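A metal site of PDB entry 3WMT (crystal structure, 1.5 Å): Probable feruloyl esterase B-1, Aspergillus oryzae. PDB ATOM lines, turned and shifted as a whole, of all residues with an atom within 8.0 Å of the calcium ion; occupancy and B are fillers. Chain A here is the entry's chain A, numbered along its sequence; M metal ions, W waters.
The calcium ion is bound by the backbone carbonyl oxygen (O) of Ile 263, the backbone carbonyl oxygen (O) of Ala 259, the side-chain carboxylate (OD1) of Asp 261, water W1, the side-chain carboxylate (OD1) of Asp 254, the backbone carbonyl oxygen (O) of Asp 254, the side-chain carboxylate (OD2) of Asp 257 and the side-chain carboxylate (OD1) of Asp 257. The calcium ion has eight donor atoms within binding distance.
The guanidinium group (NH2) of Arg 496 is in salt-bridge range of the side-chain carboxylate (OD2) of Asp 261, 3.6 Å away. OD2 of Asp 254 sits at hydrogen-bond distance from N of Gly 262, 2.8 Å away. The side-chain carboxylate (OD2) of Asp 257 sits close to the backbone NH (N) of Glu 265 (3.0 Å). The backbone carbonyl oxygen (O) of Asp 257 lies within hydrogen-bond range of the backbone NH (N) of Tyr 507, 2.8 Å away.
Water W1 bridges OD2 of Asp 261 (2.8 Å) and OE1 of Glu 265 (2.9 Å).
Within 4 Å of the calcium ion: Asp 254, Asp 257, Ala 259, Asp 261 and Ile 263.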
ATOM      1  N   ILE A 250      -6.626  12.864 -30.067  1.00  0.00           N
ATOM      2  CA  ILE A 250      -5.865  11.608 -29.793  1.00  0.00           C
ATOM      3  C   ILE A 250      -5.009  11.260 -31.028  1.00  0.00           C
ATOM      4  O   ILE A 250      -3.820  10.955 -30.959  1.00  0.00           O
ATOM      5  CB  ILE A 250      -6.817  10.461 -29.392  1.00  0.00           C
ATOM      6  CG1 ILE A 250      -7.522  10.760 -28.065  1.00  0.00           C
ATOM      7  CG2 ILE A 250      -6.092   9.096 -29.366  1.00  0.00           C
ATOM      8  CD1 ILE A 250      -6.638  10.937 -26.899  1.00  0.00           C
ATOM      9  N   CYS A 253      -2.056  13.716 -31.084  1.00  0.00           N
ATOM     10  CA  CYS A 253      -1.228  13.855 -29.859  1.00  0.00           C
ATOM     11  C   CYS A 253      -0.869  12.612 -29.136  1.00  0.00           C
ATOM     12  O   CYS A 253       0.114  12.658 -28.370  1.00  0.00           O
ATOM     13  CB  CYS A 253      -1.945  14.807 -28.936  1.00  0.00           C
ATOM     14  SG  CYS A 253      -2.040  16.459 -29.585  1.00  0.00           S
ATOM     15  N   ASP A 254      -1.559  11.494 -29.270  1.00  0.00           N
ATOM     16  CA  ASP A 254      -1.253  10.253 -28.522  1.00  0.00           C
ATOM     17  C   ASP A 254       0.243   9.866 -28.599  1.00  0.00           C
ATOM     18  O   ASP A 254       0.855   9.578 -27.541  1.00  0.00           O
ATOM     19  CB  ASP A 254      -2.170   9.139 -29.031  1.00  0.00           C
ATOM     20  CG  ASP A 254      -1.966   7.805 -28.390  1.00  0.00           C
ATOM     21  OD1 ASP A 254      -1.335   7.681 -27.306  1.00  0.00           O
ATOM     22  OD2 ASP A 254      -2.577   6.832 -28.944  1.00  0.00           O
ATOM     23  N   SER A 255       0.773   9.775 -29.788  1.00  0.00           N
ATOM     24  CA  SER A 255       2.071   9.225 -30.001  1.00  0.00           C
ATOM     25  C   SER A 255       3.179  10.162 -29.624  1.00  0.00           C
ATOM     26  O   SER A 255       4.371   9.890 -29.700  1.00  0.00           O
ATOM     27  CB  SER A 255       2.238   8.864 -31.485  1.00  0.00           C
ATOM     28  OG  SER A 255       2.278  10.050 -32.275  1.00  0.00           O
ATOM     29  N   LEU A 256       2.895  11.420 -29.217  1.00  0.00           N
ATOM     30  CA  LEU A 256       3.963  12.377 -28.890  1.00  0.00           C
ATOM     31  C   LEU A 256       4.850  11.934 -27.741  1.00  0.00           C
ATOM     32  O   LEU A 256       6.019  12.338 -27.626  1.00  0.00           O
ATOM     33  CB  LEU A 256       3.397  13.776 -28.663  1.00  0.00           C
ATOM     34  CG  LEU A 256       2.548  14.359 -29.782  1.00  0.00           C
ATOM     35  CD1 LEU A 256       2.070  15.766 -29.444  1.00  0.00           C
ATOM     36  CD2 LEU A 256       3.350  14.405 -31.114  1.00  0.00           C
ATOM     37  N   ASP A 257       4.272  11.169 -26.842  1.00  0.00           N
ATOM     38  CA  ASP A 257       4.975  10.598 -25.699  1.00  0.00           C
ATOM     39  C   ASP A 257       5.710   9.292 -26.051  1.00  0.00           C
ATOM     40  O   ASP A 257       6.325   8.716 -25.192  1.00  0.00           O
ATOM     41  CB  ASP A 257       4.020  10.389 -24.571  1.00  0.00           C
ATOM     42  CG  ASP A 257       2.836   9.614 -24.918  1.00  0.00           C
ATOM     43  OD1 ASP A 257       2.991   8.447 -25.479  1.00  0.00           O
ATOM     44  OD2 ASP A 257       1.655   9.982 -24.685  1.00  0.00           O
ATOM     45  N   GLY A 258       5.579   8.846 -27.298  1.00  0.00           N
ATOM     46  CA  GLY A 258       6.222   7.602 -27.785  1.00  0.00           C
ATOM     47  C   GLY A 258       5.254   6.456 -27.855  1.00  0.00           C
ATOM     48  O   GLY A 258       5.517   5.530 -28.679  1.00  0.00           O
ATOM     49  N   ALA A 259       4.248   6.399 -27.022  1.00  0.00           N
ATOM     50  CA  ALA A 259       3.373   5.226 -26.879  1.00  0.00           C
ATOM     51  C   ALA A 259       2.042   5.497 -27.547  1.00  0.00           C
ATOM     52  O   ALA A 259       1.331   6.450 -27.172  1.00  0.00           O
ATOM     53  CB  ALA A 259       3.181   4.899 -25.427  1.00  0.00           C
ATOM     54  N   LYS A 260       1.652   4.675 -28.520  1.00  0.00           N
ATOM     55  CA  LYS A 260       0.336   4.724 -29.163  1.00  0.00           C
ATOM     56  C   LYS A 260      -0.619   3.876 -28.331  1.00  0.00           C
ATOM     57  O   LYS A 260      -0.938   2.701 -28.635  1.00  0.00           O
ATOM     58  CB  LYS A 260       0.410   4.290 -30.641  1.00  0.00           C
ATOM     59  CG  LYS A 260      -0.919   4.566 -31.336  1.00  0.00           C
ATOM     60  CD  LYS A 260      -0.873   4.143 -32.822  1.00  0.00           C
ATOM     61  CE  LYS A 260      -2.110   4.626 -33.526  1.00  0.00           C
ATOM     62  NZ  LYS A 260      -3.314   4.026 -32.945  1.00  0.00           N
ATOM     63  N   ASP A 261      -1.044   4.436 -27.180  1.00  0.00           N
ATOM     64  CA  ASP A 261      -1.810   3.784 -26.162  1.00  0.00           C
ATOM     65  C   ASP A 261      -3.145   4.460 -25.863  1.00  0.00           C
ATOM     66  O   ASP A 261      -3.806   4.155 -24.907  1.00  0.00           O
ATOM     67  CB  ASP A 261      -0.994   3.648 -24.882  1.00  0.00           C
ATOM     68  CG  ASP A 261      -0.562   4.990 -24.297  1.00  0.00           C
ATOM     69  OD1 ASP A 261      -0.765   6.013 -24.981  1.00  0.00           O
ATOM     70  OD2 ASP A 261      -0.096   4.997 -23.138  1.00  0.00           O
ATOM     71  N   GLY A 262      -3.539   5.442 -26.704  1.00  0.00           N
ATOM     72  CA  GLY A 262      -4.696   6.167 -26.502  1.00  0.00           C
ATOM     73  C   GLY A 262      -4.639   7.300 -25.414  1.00  0.00           C
ATOM     74  O   GLY A 262      -5.689   7.931 -25.118  1.00  0.00           O
ATOM     75  N   ILE A 263      -3.461   7.534 -24.860  1.00  0.00           N
ATOM     76  CA  ILE A 263      -3.271   8.456 -23.720  1.00  0.00           C
ATOM     77  C   ILE A 263      -2.316   9.505 -24.139  1.00  0.00           C
ATOM     78  O   ILE A 263      -1.286   9.268 -24.802  1.00  0.00           O
ATOM     79  CB  ILE A 263      -2.703   7.676 -22.550  1.00  0.00           C
ATOM     80  CG1 ILE A 263      -3.797   6.702 -22.050  1.00  0.00           C
ATOM     81  CG2 ILE A 263      -2.330   8.586 -21.373  1.00  0.00           C
ATOM     82  CD1 ILE A 263      -3.329   5.608 -21.188  1.00  0.00           C
ATOM     83  N   ILE A 264      -2.615  10.769 -23.746  1.00  0.00           N
ATOM     84  CA  ILE A 264      -1.753  11.877 -23.953  1.00  0.00           C
ATOM     85  C   ILE A 264      -0.971  12.060 -22.644  1.00  0.00           C
ATOM     86  O   ILE A 264      -1.454  12.590 -21.656  1.00  0.00           O
ATOM     87  CB  ILE A 264      -2.438  13.190 -24.353  1.00  0.00           C
ATOM     88  CG1 ILE A 264      -3.281  12.946 -25.607  1.00  0.00           C
ATOM     89  CG2 ILE A 264      -1.456  14.271 -24.575  1.00  0.00           C
ATOM     90  CD1 ILE A 264      -4.245  14.083 -25.937  1.00  0.00           C
ATOM     91  N   GLU A 265       0.261  11.540 -22.583  1.00  0.00           N
ATOM     92  CA  GLU A 265       1.002  11.474 -21.340  1.00  0.00           C
ATOM     93  C   GLU A 265       1.243  12.872 -20.733  1.00  0.00           C
ATOM     94  O   GLU A 265       1.028  13.068 -19.538  1.00  0.00           O
ATOM     95  CB  GLU A 265       2.313  10.733 -21.508  1.00  0.00           C
ATOM     96  CG  GLU A 265       2.855  10.153 -20.252  1.00  0.00           C
ATOM     97  CD  GLU A 265       2.164   8.913 -19.765  1.00  0.00           C
ATOM     98  OE1 GLU A 265       1.359   8.333 -20.515  1.00  0.00           O
ATOM     99  OE2 GLU A 265       2.434   8.510 -18.580  1.00  0.00           O
ATOM    100  N   ASP A 266       1.639  13.833 -21.597  1.00  0.00           N
ATOM    101  CA  ASP A 266       1.912  15.206 -21.180  1.00  0.00           C
ATOM    102  C   ASP A 266       1.279  16.114 -22.209  1.00  0.00           C
ATOM    103  O   ASP A 266       1.823  16.377 -23.286  1.00  0.00           O
ATOM    104  CB  ASP A 266       3.409  15.445 -21.109  1.00  0.00           C
ATOM    105  CG  ASP A 266       3.835  16.829 -20.849  1.00  0.00           C
ATOM    106  OD1 ASP A 266       2.967  17.717 -20.747  1.00  0.00           O
ATOM    107  OD2 ASP A 266       5.090  17.064 -20.671  1.00  0.00           O
ATOM    108  N   ARG A 496       2.589   2.556 -13.907  1.00  0.00           N
ATOM    109  CA  ARG A 496       3.552   3.459 -14.461  1.00  0.00           C
ATOM    110  C   ARG A 496       4.052   4.347 -13.392  1.00  0.00           C
ATOM    111  O   ARG A 496       3.283   4.828 -12.542  1.00  0.00           O
ATOM    112  CB  ARG A 496       2.955   4.322 -15.604  1.00  0.00           C
ATOM    113  CG  ARG A 496       3.913   5.243 -16.307  1.00  0.00           C
ATOM    114  CD  ARG A 496       3.907   5.191 -17.800  1.00  0.00           C
ATOM    115  NE  ARG A 496       2.698   5.707 -18.394  1.00  0.00           N
ATOM    116  CZ  ARG A 496       1.828   5.023 -19.127  1.00  0.00           C
ATOM    117  NH1 ARG A 496       1.849   3.692 -19.176  1.00  0.00           N
ATOM    118  NH2 ARG A 496       0.874   5.610 -19.778  1.00  0.00           N
ATOM    119  N   TYR A 507       8.133   7.219 -23.578  1.00  0.00           N
ATOM    120  CA  TYR A 507       8.081   5.744 -23.842  1.00  0.00           C
ATOM    121  C   TYR A 507       9.249   5.450 -24.799  1.00  0.00           C
ATOM    122  O   TYR A 507       9.325   6.038 -25.880  1.00  0.00           O
ATOM    123  CB  TYR A 507       6.780   5.300 -24.389  1.00  0.00           C
ATOM    124  CG  TYR A 507       6.777   3.868 -24.857  1.00  0.00           C
ATOM    125  CD1 TYR A 507       6.929   2.808 -24.017  1.00  0.00           C
ATOM    126  CD2 TYR A 507       6.716   3.634 -26.223  1.00  0.00           C
ATOM    127  CE1 TYR A 507       6.958   1.499 -24.509  1.00  0.00           C
ATOM    128  CE2 TYR A 507       6.756   2.309 -26.731  1.00  0.00           C
ATOM    129  CZ  TYR A 507       6.907   1.290 -25.862  1.00  0.00           C
ATOM    130  OH  TYR A 507       6.967  -0.023 -26.301  1.00  0.00           O
ATOM    131  N   TYR A 513       4.393  -0.552 -23.747  1.00  0.00           N
ATOM    132  CA  TYR A 513       4.130   0.617 -22.877  1.00  0.00           C
ATOM    133  C   TYR A 513       3.506   0.211 -21.553  1.00  0.00           C
ATOM    134  O   TYR A 513       3.481   1.053 -20.629  1.00  0.00           O
ATOM    135  CB  TYR A 513       3.276   1.628 -23.590  1.00  0.00           C
ATOM    136  CG  TYR A 513       1.923   1.111 -24.134  1.00  0.00           C
ATOM    137  CD1 TYR A 513       0.861   0.843 -23.302  1.00  0.00           C
ATOM    138  CD2 TYR A 513       1.758   0.949 -25.518  1.00  0.00           C
ATOM    139  CE1 TYR A 513      -0.342   0.356 -23.834  1.00  0.00           C
ATOM    140  CE2 TYR A 513       0.574   0.470 -26.039  1.00  0.00           C
ATOM    141  CZ  TYR A 513      -0.446   0.188 -25.184  1.00  0.00           C
ATOM    142  OH  TYR A 513      -1.739  -0.202 -25.612  1.00  0.00           O
ATOM    143  N   TRP A 519       9.591   3.139 -19.879  1.00  0.00           N
ATOM    144  CA  TRP A 519       9.454   4.599 -19.802  1.00  0.00           C
ATOM    145  C   TRP A 519      10.592   5.186 -19.098  1.00  0.00           C
ATOM    146  O   TRP A 519      11.131   4.581 -18.143  1.00  0.00           O
ATOM    147  CB  TRP A 519       8.174   4.973 -19.093  1.00  0.00           C
ATOM    148  CG  TRP A 519       6.911   4.567 -19.774  1.00  0.00           C
ATOM    149  CD1 TRP A 519       6.298   3.331 -19.836  1.00  0.00           C
ATOM    150  CD2 TRP A 519       6.044   5.424 -20.568  1.00  0.00           C
ATOM    151  NE1 TRP A 519       5.160   3.385 -20.591  1.00  0.00           N
ATOM    152  CE2 TRP A 519       4.977   4.679 -21.027  1.00  0.00           C
ATOM    153  CE3 TRP A 519       6.119   6.800 -20.892  1.00  0.00           C
ATOM    154  CZ2 TRP A 519       3.927   5.252 -21.769  1.00  0.00           C
ATOM    155  CZ3 TRP A 519       5.095   7.336 -21.595  1.00  0.00           C
ATOM    156  CH2 TRP A 519       4.049   6.527 -22.079  1.00  0.00           C
HETATM  157 CA    CA M   1       0.448   8.036 -25.653  1.00  0.00          CA
HETATM  158  O   HOH W   1       0.922   7.549 -23.294  1.00  0.00           O
